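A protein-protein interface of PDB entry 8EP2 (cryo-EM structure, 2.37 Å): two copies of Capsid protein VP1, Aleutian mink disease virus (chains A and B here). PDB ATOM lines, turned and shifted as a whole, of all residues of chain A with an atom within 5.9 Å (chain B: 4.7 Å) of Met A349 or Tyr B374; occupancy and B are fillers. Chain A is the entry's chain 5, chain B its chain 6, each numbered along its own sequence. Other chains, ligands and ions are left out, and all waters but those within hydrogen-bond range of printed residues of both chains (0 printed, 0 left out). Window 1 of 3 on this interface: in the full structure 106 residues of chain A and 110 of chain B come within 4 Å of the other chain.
The side-chain sulfur (SD) of Met A349 sits close to the side-chain hydroxyl (OG) of Ser B373 (3.5 Å).
O of Ser B373 sits at hydrogen-bond distance from NH1 of Arg A296.
N of Phe B375 lies close to O of Met A349 (3.2 Å).
O of Ala B376 lies within hydrogen-bond range of ND2 of Asn A356 (3.1 Å).
The side-chain carboxylate (OD2) of Asp B104 lies within salt-bridge range of the guanidinium group (NH1) of Arg A296, at 3.2 Å.
The side-chain sulfur of Met A349 lies close to the backbone carbonyl oxygen of Phe B101, at 3.6 Å.
The side-chain sulfur (SD) of Met A349 sits close to the side-chain carboxylate (OD1) of Asp B104, 3.5 Å away.
NE2 of His A471 lies within hydrogen-bond range of OH of Tyr B374 (3.0 Å).
O of Pro B367 is in hydrogen-bond range of N of Tyr B374, 3.0 Å away.
The backbone carbonyl oxygen (O) of Thr A295 is in hydrogen-bond range of the guanidinium group (NE) of Arg A353, 3.4 Å away.
The backbone carbonyl oxygen of Ala A347 lies close to the side-chain amide oxygen of Asn A350 (3.0 Å).
O of Asn A350 is in hydrogen-bond range of N of Trp A338, 3.1 Å away.
The backbone carbonyl oxygen of Ile B365 is in hydrogen-bond range of the backbone NH of Ala B376, 3.4 Å away.
OE2 of Glu A348 lies within salt-bridge range of NH2 of Arg A353 (3.9 Å).
Among the printed residues, pairs that only touch across the chains: Thr A295 with Tyr B374 (3.0 Å), Asn A350 with Phe B375 (3.4 Å), Arg A296 with Gly B372 (3.4 Å), Glu A348 with Asp B104 (3.5 Å), Met A349 with Ile B366 (3.5 Å), His A471 with Pro B367 (3.5 Å), Asn A356 with Tyr B374 (3.6 Å), Ala A347 with Val B102 (3.6 Å), Ala A347 with Asp B104 (3.7 Å), Met A349 with Tyr B374 (3.7 Å), Met A349 with Val B102 (3.8 Å) and Trp A338 with Phe B375 (3.9 Å).
Of chain B, only Phe B101 (3.5 Å), Val B102 (3.8 Å), Asp B104 (3.4 Å), Ile B366 (3.5 Å), Ser B373 (3.3 Å), Tyr B374 (3.7 Å) and Phe B375 (3.1 Å) come within 4 Å of Met A349.
Printed residues of chain A within 4 Å of Val B102: Ala A347 and Met A349.
Of the printed residues of chain A, Asp B104 touches Arg A296, Ala A347, Glu A348 and Met A349.
Tyr B374 touches four residues of chain A.
Of the printed residues of chain A, Phe B375 touches Trp A338 (3.9 Å), Met A349 (3.1 Å) and Asn A350 (3.4 Å).
The nearest residue of chain A that does not touch Tyr B374 is Arg A296 (4.2 Å).
Of the 12 printed residues of chain B, 10 touch a printed residue of chain A.
Of the 16 printed residues of chain A, 9 touch a printed residue of chain B.
Hydrophobic or aromatic side chains of chain A that line the printed part of chain B: Trp A338, Ala A347, Met A349 and His A471.
Among the printed residues, Asp or Glu carboxylates within 4 Å of a Lys or Arg side-chain nitrogen of the other chain: Arg A296 with Asp B104 (3.2 Å).
No position is printed for both chains.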
ATOM      1  N   THR A 295      13.334  11.181 -17.926  1.00  0.00           N
ATOM      2  CA  THR A 295      14.469  10.876 -18.783  1.00  0.00           C
ATOM      3  C   THR A 295      15.381   9.836 -18.148  1.00  0.00           C
ATOM      4  O   THR A 295      15.936   8.983 -18.845  1.00  0.00           O
ATOM      5  CB  THR A 295      15.252  12.143 -19.081  1.00  0.00           C
ATOM      6  OG1 THR A 295      15.805  12.620 -17.861  1.00  0.00           O
ATOM      7  CG2 THR A 295      14.342  13.198 -19.616  1.00  0.00           C
ATOM      8  N   ARG A 296      15.549   9.886 -16.828  1.00  0.00           N
ATOM      9  CA  ARG A 296      16.400   8.920 -16.147  1.00  0.00           C
ATOM     10  C   ARG A 296      15.919   7.488 -16.315  1.00  0.00           C
ATOM     11  O   ARG A 296      16.702   6.561 -16.110  1.00  0.00           O
ATOM     12  CB  ARG A 296      16.490   9.253 -14.659  1.00  0.00           C
ATOM     13  CG  ARG A 296      17.279  10.496 -14.328  1.00  0.00           C
ATOM     14  CD  ARG A 296      18.755  10.262 -14.502  1.00  0.00           C
ATOM     15  NE  ARG A 296      19.254   9.308 -13.522  1.00  0.00           N
ATOM     16  CZ  ARG A 296      19.679   9.644 -12.312  1.00  0.00           C
ATOM     17  NH1 ARG A 296      19.699  10.911 -11.946  1.00  0.00           N
ATOM     18  NH2 ARG A 296      20.101   8.717 -11.476  1.00  0.00           N
ATOM     19  N   ARG A 333      32.035   2.600 -16.619  1.00  0.00           N
ATOM     20  CA  ARG A 333      30.980   1.914 -17.342  1.00  0.00           C
ATOM     21  C   ARG A 333      31.280   1.982 -18.828  1.00  0.00           C
ATOM     22  O   ARG A 333      32.024   2.849 -19.282  1.00  0.00           O
ATOM     23  CB  ARG A 333      29.621   2.550 -17.062  1.00  0.00           C
ATOM     24  CG  ARG A 333      29.190   2.458 -15.626  1.00  0.00           C
ATOM     25  CD  ARG A 333      27.928   3.238 -15.383  1.00  0.00           C
ATOM     26  NE  ARG A 333      26.824   2.736 -16.183  1.00  0.00           N
ATOM     27  CZ  ARG A 333      25.620   3.287 -16.218  1.00  0.00           C
ATOM     28  NH1 ARG A 333      24.677   2.769 -16.978  1.00  0.00           N
ATOM     29  NH2 ARG A 333      25.363   4.351 -15.481  1.00  0.00           N
ATOM     30  N   TRP A 338      27.663  12.080 -22.509  1.00  0.00           N
ATOM     31  CA  TRP A 338      27.973  13.468 -22.809  1.00  0.00           C
ATOM     32  C   TRP A 338      29.324  13.841 -22.219  1.00  0.00           C
ATOM     33  O   TRP A 338      29.689  13.385 -21.135  1.00  0.00           O
ATOM     34  CB  TRP A 338      26.909  14.401 -22.240  1.00  0.00           C
ATOM     35  CG  TRP A 338      25.549  14.268 -22.824  1.00  0.00           C
ATOM     36  CD1 TRP A 338      24.483  13.653 -22.260  1.00  0.00           C
ATOM     37  CD2 TRP A 338      25.111  14.743 -24.093  1.00  0.00           C
ATOM     38  NE1 TRP A 338      23.402  13.728 -23.087  1.00  0.00           N
ATOM     39  CE2 TRP A 338      23.761  14.391 -24.224  1.00  0.00           C
ATOM     40  CE3 TRP A 338      25.729  15.437 -25.130  1.00  0.00           C
ATOM     41  CZ2 TRP A 338      23.020  14.705 -25.349  1.00  0.00           C
ATOM     42  CZ3 TRP A 338      24.991  15.748 -26.239  1.00  0.00           C
ATOM     43  CH2 TRP A 338      23.651  15.384 -26.343  1.00  0.00           C
ATOM     44  N   ALA A 347      28.300   8.237 -15.291  1.00  0.00           N
ATOM     45  CA  ALA A 347      27.257   7.740 -14.418  1.00  0.00           C
ATOM     46  C   ALA A 347      25.926   7.777 -15.141  1.00  0.00           C
ATOM     47  O   ALA A 347      25.827   8.163 -16.304  1.00  0.00           O
ATOM     48  CB  ALA A 347      27.187   8.548 -13.123  1.00  0.00           C
ATOM     49  N   GLU A 348      24.895   7.398 -14.413  1.00  0.00           N
ATOM     50  CA  GLU A 348      23.546   7.358 -14.926  1.00  0.00           C
ATOM     51  C   GLU A 348      23.023   8.734 -15.273  1.00  0.00           C
ATOM     52  O   GLU A 348      22.010   8.863 -15.936  1.00  0.00           O
ATOM     53  CB  GLU A 348      22.654   6.773 -13.840  1.00  0.00           C
ATOM     54  CG  GLU A 348      21.367   6.176 -14.339  1.00  0.00           C
ATOM     55  CD  GLU A 348      21.611   4.943 -15.167  1.00  0.00           C
ATOM     56  OE1 GLU A 348      22.700   4.823 -15.755  1.00  0.00           O
ATOM     57  OE2 GLU A 348      20.714   4.091 -15.227  1.00  0.00           O
ATOM     58  N   MET A 349      23.742   9.766 -14.859  1.00  0.00           N
ATOM     59  CA  MET A 349      23.281  11.131 -15.038  1.00  0.00           C
ATOM     60  C   MET A 349      23.667  11.707 -16.395  1.00  0.00           C
ATOM     61  O   MET A 349      22.867  12.413 -17.012  1.00  0.00           O
ATOM     62  CB  MET A 349      23.825  11.986 -13.905  1.00  0.00           C
ATOM     63  CG  MET A 349      23.403  13.409 -13.952  1.00  0.00           C
ATOM     64  SD  MET A 349      23.829  14.200 -12.409  1.00  0.00           S
ATOM     65  CE  MET A 349      23.503  15.878 -12.862  1.00  0.00           C
ATOM     66  N   ASN A 350      24.880  11.449 -16.874  1.00  0.00           N
ATOM     67  CA  ASN A 350      25.285  11.912 -18.196  1.00  0.00           C
ATOM     68  C   ASN A 350      25.116  10.864 -19.282  1.00  0.00           C
ATOM     69  O   ASN A 350      25.527  11.100 -20.417  1.00  0.00           O
ATOM     70  CB  ASN A 350      26.728  12.415 -18.188  1.00  0.00           C
ATOM     71  CG  ASN A 350      27.710  11.373 -17.746  1.00  0.00           C
ATOM     72  OD1 ASN A 350      27.465  10.184 -17.846  1.00  0.00           O
ATOM     73  ND2 ASN A 350      28.857  11.818 -17.291  1.00  0.00           N
ATOM     74  N   ARG A 351      24.557   9.710 -18.955  1.00  0.00           N
ATOM     75  CA  ARG A 351      24.206   8.734 -19.972  1.00  0.00           C
ATOM     76  C   ARG A 351      23.292   9.375 -21.006  1.00  0.00           C
ATOM     77  O   ARG A 351      22.260   9.948 -20.662  1.00  0.00           O
ATOM     78  CB  ARG A 351      23.507   7.556 -19.311  1.00  0.00           C
ATOM     79  CG  ARG A 351      23.153   6.440 -20.231  1.00  0.00           C
ATOM     80  CD  ARG A 351      22.354   5.404 -19.489  1.00  0.00           C
ATOM     81  NE  ARG A 351      22.035   4.255 -20.320  1.00  0.00           N
ATOM     82  CZ  ARG A 351      21.046   4.223 -21.205  1.00  0.00           C
ATOM     83  NH1 ARG A 351      20.828   3.128 -21.910  1.00  0.00           N
ATOM     84  NH2 ARG A 351      20.301   5.294 -21.417  1.00  0.00           N
ATOM     85  N   ARG A 353      20.509   9.949 -23.552  1.00  0.00           N
ATOM     86  CA  ARG A 353      19.171   9.433 -23.651  1.00  0.00           C
ATOM     87  C   ARG A 353      18.586   9.811 -25.001  1.00  0.00           C
ATOM     88  O   ARG A 353      19.026  10.780 -25.619  1.00  0.00           O
ATOM     89  CB  ARG A 353      18.294  10.017 -22.547  1.00  0.00           C
ATOM     90  CG  ARG A 353      18.821   9.806 -21.156  1.00  0.00           C
ATOM     91  CD  ARG A 353      18.708   8.393 -20.659  1.00  0.00           C
ATOM     92  NE  ARG A 353      19.202   8.321 -19.290  1.00  0.00           N
ATOM     93  CZ  ARG A 353      19.276   7.212 -18.568  1.00  0.00           C
ATOM     94  NH1 ARG A 353      18.855   6.067 -19.065  1.00  0.00           N
ATOM     95  NH2 ARG A 353      19.745   7.258 -17.339  1.00  0.00           N
ATOM     96  N   TYR A 355      15.699  11.124 -25.719  1.00  0.00           N
ATOM     97  CA  TYR A 355      14.768  12.235 -25.701  1.00  0.00           C
ATOM     98  C   TYR A 355      14.886  12.952 -24.371  1.00  0.00           C
ATOM     99  O   TYR A 355      15.499  12.454 -23.430  1.00  0.00           O
ATOM    100  CB  TYR A 355      13.335  11.742 -25.876  1.00  0.00           C
ATOM    101  CG  TYR A 355      13.127  10.920 -27.106  1.00  0.00           C
ATOM    102  CD1 TYR A 355      13.438  11.410 -28.355  1.00  0.00           C
ATOM    103  CD2 TYR A 355      12.685   9.622 -27.008  1.00  0.00           C
ATOM    104  CE1 TYR A 355      13.267  10.650 -29.468  1.00  0.00           C
ATOM    105  CE2 TYR A 355      12.523   8.853 -28.111  1.00  0.00           C
ATOM    106  CZ  TYR A 355      12.808   9.368 -29.338  1.00  0.00           C
ATOM    107  OH  TYR A 355      12.637   8.589 -30.450  1.00  0.00           O
ATOM    108  N   ASN A 356      14.295  14.132 -24.305  1.00  0.00           N
ATOM    109  CA  ASN A 356      14.048  14.824 -23.051  1.00  0.00           C
ATOM    110  C   ASN A 356      12.553  14.833 -22.798  1.00  0.00           C
ATOM    111  O   ASN A 356      11.773  15.175 -23.687  1.00  0.00           O
ATOM    112  CB  ASN A 356      14.580  16.252 -23.087  1.00  0.00           C
ATOM    113  CG  ASN A 356      16.071  16.307 -23.042  1.00  0.00           C
ATOM    114  OD1 ASN A 356      16.720  15.387 -22.563  1.00  0.00           O
ATOM    115  ND2 ASN A 356      16.633  17.388 -23.536  1.00  0.00           N
ATOM    116  N   ILE A 357      12.155  14.456 -21.597  1.00  0.00           N
ATOM    117  CA  ILE A 357      10.750  14.347 -21.244  1.00  0.00           C
ATOM    118  C   ILE A 357      10.387  15.567 -20.416  1.00  0.00           C
ATOM    119  O   ILE A 357      10.853  15.723 -19.286  1.00  0.00           O
ATOM    120  CB  ILE A 357      10.470  13.040 -20.501  1.00  0.00           C
ATOM    121  CG1 ILE A 357      10.749  11.879 -21.441  1.00  0.00           C
ATOM    122  CG2 ILE A 357       9.044  12.988 -20.043  1.00  0.00           C
ATOM    123  CD1 ILE A 357      10.739  10.574 -20.775  1.00  0.00           C
ATOM    124  N   GLY A 358       9.562  16.435 -20.983  1.00  0.00           N
ATOM    125  CA  GLY A 358       9.270  17.707 -20.370  1.00  0.00           C
ATOM    126  C   GLY A 358      10.418  18.674 -20.536  1.00  0.00           C
ATOM    127  O   GLY A 358      11.475  18.349 -21.065  1.00  0.00           O
ATOM    128  N   TYR A 359      10.201  19.895 -20.070  1.00  0.00           N
ATOM    129  CA  TYR A 359      11.247  20.896 -20.154  1.00  0.00           C
ATOM    130  C   TYR A 359      11.038  21.936 -19.070  1.00  0.00           C
ATOM    131  O   TYR A 359       9.935  22.115 -18.557  1.00  0.00           O
ATOM    132  CB  TYR A 359      11.286  21.543 -21.540  1.00  0.00           C
ATOM    133  CG  TYR A 359      10.023  22.251 -21.929  1.00  0.00           C
ATOM    134  CD1 TYR A 359       9.876  23.606 -21.728  1.00  0.00           C
ATOM    135  CD2 TYR A 359       8.966  21.555 -22.479  1.00  0.00           C
ATOM    136  CE1 TYR A 359       8.726  24.247 -22.080  1.00  0.00           C
ATOM    137  CE2 TYR A 359       7.814  22.187 -22.828  1.00  0.00           C
ATOM    138  CZ  TYR A 359       7.695  23.531 -22.629  1.00  0.00           C
ATOM    139  OH  TYR A 359       6.533  24.162 -22.982  1.00  0.00           O
ATOM    140  N   HIS A 471       9.396  19.096 -13.626  1.00  0.00           N
ATOM    141  CA  HIS A 471      10.738  19.528 -13.287  1.00  0.00           C
ATOM    142  C   HIS A 471      10.682  20.339 -12.009  1.00  0.00           C
ATOM    143  O   HIS A 471       9.735  21.086 -11.772  1.00  0.00           O
ATOM    144  CB  HIS A 471      11.356  20.356 -14.408  1.00  0.00           C
ATOM    145  CG  HIS A 471      11.724  19.550 -15.608  1.00  0.00           C
ATOM    146  ND1 HIS A 471      10.791  19.088 -16.509  1.00  0.00           N
ATOM    147  CD2 HIS A 471      12.924  19.125 -16.059  1.00  0.00           C
ATOM    148  CE1 HIS A 471      11.401  18.403 -17.456  1.00  0.00           C
ATOM    149  NE2 HIS A 471      12.697  18.415 -17.209  1.00  0.00           N
ATOM    150  N   PHE B 101      27.682  14.755  -6.670  1.00  0.00           N
ATOM    151  CA  PHE B 101      26.488  15.199  -7.373  1.00  0.00           C
ATOM    152  C   PHE B 101      26.346  14.537  -8.734  1.00  0.00           C
ATOM    153  O   PHE B 101      25.264  14.064  -9.093  1.00  0.00           O
ATOM    154  CB  PHE B 101      26.487  16.711  -7.525  1.00  0.00           C
ATOM    155  CG  PHE B 101      25.307  17.211  -8.268  1.00  0.00           C
ATOM    156  CD1 PHE B 101      24.080  17.296  -7.647  1.00  0.00           C
ATOM    157  CD2 PHE B 101      25.408  17.570  -9.593  1.00  0.00           C
ATOM    158  CE1 PHE B 101      22.981  17.739  -8.329  1.00  0.00           C
ATOM    159  CE2 PHE B 101      24.310  18.018 -10.274  1.00  0.00           C
ATOM    160  CZ  PHE B 101      23.096  18.100  -9.639  1.00  0.00           C
ATOM    161  N   VAL B 102      27.419  14.504  -9.526  1.00  0.00           N
ATOM    162  CA  VAL B 102      27.279  14.007 -10.889  1.00  0.00           C
ATOM    163  C   VAL B 102      27.423  12.502 -11.006  1.00  0.00           C
ATOM    164  O   VAL B 102      27.182  11.958 -12.086  1.00  0.00           O
ATOM    165  CB  VAL B 102      28.301  14.648 -11.842  1.00  0.00           C
ATOM    166  CG1 VAL B 102      28.088  16.136 -11.912  1.00  0.00           C
ATOM    167  CG2 VAL B 102      29.704  14.328 -11.398  1.00  0.00           C
ATOM    168  N   ASP B 104      25.685  10.082  -9.331  1.00  0.00           N
ATOM    169  CA  ASP B 104      24.559   9.228  -8.962  1.00  0.00           C
ATOM    170  C   ASP B 104      24.224   8.242 -10.068  1.00  0.00           C
ATOM    171  O   ASP B 104      23.997   8.626 -11.218  1.00  0.00           O
ATOM    172  CB  ASP B 104      23.322  10.050  -8.610  1.00  0.00           C
ATOM    173  CG  ASP B 104      22.955  11.016  -9.667  1.00  0.00           C
ATOM    174  OD1 ASP B 104      23.777  11.224 -10.577  1.00  0.00           O
ATOM    175  OD2 ASP B 104      21.837  11.570  -9.600  1.00  0.00           O
ATOM    176  N   ILE B 365      23.545  22.357 -18.843  1.00  0.00           N
ATOM    177  CA  ILE B 365      22.514  22.576 -17.839  1.00  0.00           C
ATOM    178  C   ILE B 365      21.930  21.222 -17.477  1.00  0.00           C
ATOM    179  O   ILE B 365      21.677  20.391 -18.355  1.00  0.00           O
ATOM    180  CB  ILE B 365      21.424  23.529 -18.350  1.00  0.00           C
ATOM    181  CG1 ILE B 365      20.754  22.965 -19.591  1.00  0.00           C
ATOM    182  CG2 ILE B 365      21.999  24.883 -18.662  1.00  0.00           C
ATOM    183  CD1 ILE B 365      19.587  23.763 -20.037  1.00  0.00           C
ATOM    184  N   ILE B 366      21.761  20.969 -16.187  1.00  0.00           N
ATOM    185  CA  ILE B 366      21.119  19.720 -15.807  1.00  0.00           C
ATOM    186  C   ILE B 366      19.818  20.041 -15.081  1.00  0.00           C
ATOM    187  O   ILE B 366      19.825  20.619 -13.991  1.00  0.00           O
ATOM    188  CB  ILE B 366      22.075  18.816 -15.008  1.00  0.00           C
ATOM    189  CG1 ILE B 366      22.452  19.407 -13.666  1.00  0.00           C
ATOM    190  CG2 ILE B 366      23.364  18.625 -15.762  1.00  0.00           C
ATOM    191  CD1 ILE B 366      21.666  18.824 -12.530  1.00  0.00           C
ATOM    192  N   PRO B 367      18.682  19.773 -15.699  1.00  0.00           N
ATOM    193  CA  PRO B 367      17.412  19.854 -14.985  1.00  0.00           C
ATOM    194  C   PRO B 367      17.191  18.641 -14.099  1.00  0.00           C
ATOM    195  O   PRO B 367      17.857  17.615 -14.219  1.00  0.00           O
ATOM    196  CB  PRO B 367      16.384  19.917 -16.112  1.00  0.00           C
ATOM    197  CG  PRO B 367      17.045  19.269 -17.237  1.00  0.00           C
ATOM    198  CD  PRO B 367      18.493  19.545 -17.136  1.00  0.00           C
ATOM    199  N   GLY B 369      14.396  15.962 -13.030  1.00  0.00           N
ATOM    200  CA  GLY B 369      13.126  15.309 -13.264  1.00  0.00           C
ATOM    201  C   GLY B 369      12.674  14.535 -12.046  1.00  0.00           C
ATOM    202  O   GLY B 369      13.296  14.575 -10.983  1.00  0.00           O
ATOM    203  N   GLY B 372      15.381  11.788 -11.206  1.00  0.00           N
ATOM    204  CA  GLY B 372      16.735  12.241 -10.984  1.00  0.00           C
ATOM    205  C   GLY B 372      17.055  13.424 -11.861  1.00  0.00           C
ATOM    206  O   GLY B 372      16.298  13.799 -12.747  1.00  0.00           O
ATOM    207  N   SER B 373      18.208  14.010 -11.592  1.00  0.00           N
ATOM    208  CA  SER B 373      18.729  15.052 -12.449  1.00  0.00           C
ATOM    209  C   SER B 373      19.473  14.429 -13.618  1.00  0.00           C
ATOM    210  O   SER B 373      20.036  13.341 -13.509  1.00  0.00           O
ATOM    211  CB  SER B 373      19.633  15.987 -11.661  1.00  0.00           C
ATOM    212  OG  SER B 373      20.740  15.288 -11.143  1.00  0.00           O
ATOM    213  N   TYR B 374      19.444  15.112 -14.754  1.00  0.00           N
ATOM    214  CA  TYR B 374      19.996  14.557 -15.976  1.00  0.00           C
ATOM    215  C   TYR B 374      20.579  15.672 -16.820  1.00  0.00           C
ATOM    216  O   TYR B 374      20.142  16.818 -16.747  1.00  0.00           O
ATOM    217  CB  TYR B 374      18.927  13.810 -16.771  1.00  0.00           C
ATOM    218  CG  TYR B 374      17.847  14.709 -17.309  1.00  0.00           C
ATOM    219  CD1 TYR B 374      17.920  15.213 -18.591  1.00  0.00           C
ATOM    220  CD2 TYR B 374      16.774  15.079 -16.522  1.00  0.00           C
ATOM    221  CE1 TYR B 374      16.951  16.035 -19.079  1.00  0.00           C
ATOM    222  CE2 TYR B 374      15.798  15.902 -17.004  1.00  0.00           C
ATOM    223  CZ  TYR B 374      15.891  16.374 -18.285  1.00  0.00           C
ATOM    224  OH  TYR B 374      14.914  17.203 -18.775  1.00  0.00           O
ATOM    225  N   PHE B 375      21.562  15.321 -17.632  1.00  0.00           N
ATOM    226  CA  PHE B 375      22.111  16.241 -18.615  1.00  0.00           C
ATOM    227  C   PHE B 375      21.134  16.382 -19.769  1.00  0.00           C
ATOM    228  O   PHE B 375      20.721  15.388 -20.364  1.00  0.00           O
ATOM    229  CB  PHE B 375      23.461  15.733 -19.101  1.00  0.00           C
ATOM    230  CG  PHE B 375      24.541  15.840 -18.079  1.00  0.00           C
ATOM    231  CD1 PHE B 375      25.449  16.858 -18.126  1.00  0.00           C
ATOM    232  CD2 PHE B 375      24.595  14.978 -17.017  1.00  0.00           C
ATOM    233  CE1 PHE B 375      26.437  16.961 -17.184  1.00  0.00           C
ATOM    234  CE2 PHE B 375      25.576  15.087 -16.072  1.00  0.00           C
ATOM    235  CZ  PHE B 375      26.490  16.083 -16.156  1.00  0.00           C
ATOM    236  N   ALA B 376      20.761  17.618 -20.086  1.00  0.00           N
ATOM    237  CA  ALA B 376      19.809  17.841 -21.160  1.00  0.00           C
ATOM    238  C   ALA B 376      20.449  17.726 -22.531  1.00  0.00           C
ATOM    239  O   ALA B 376      19.733  17.580 -23.523  1.00  0.00           O
ATOM    240  CB  ALA B 376      19.162  19.211 -21.013  1.00  0.00           C
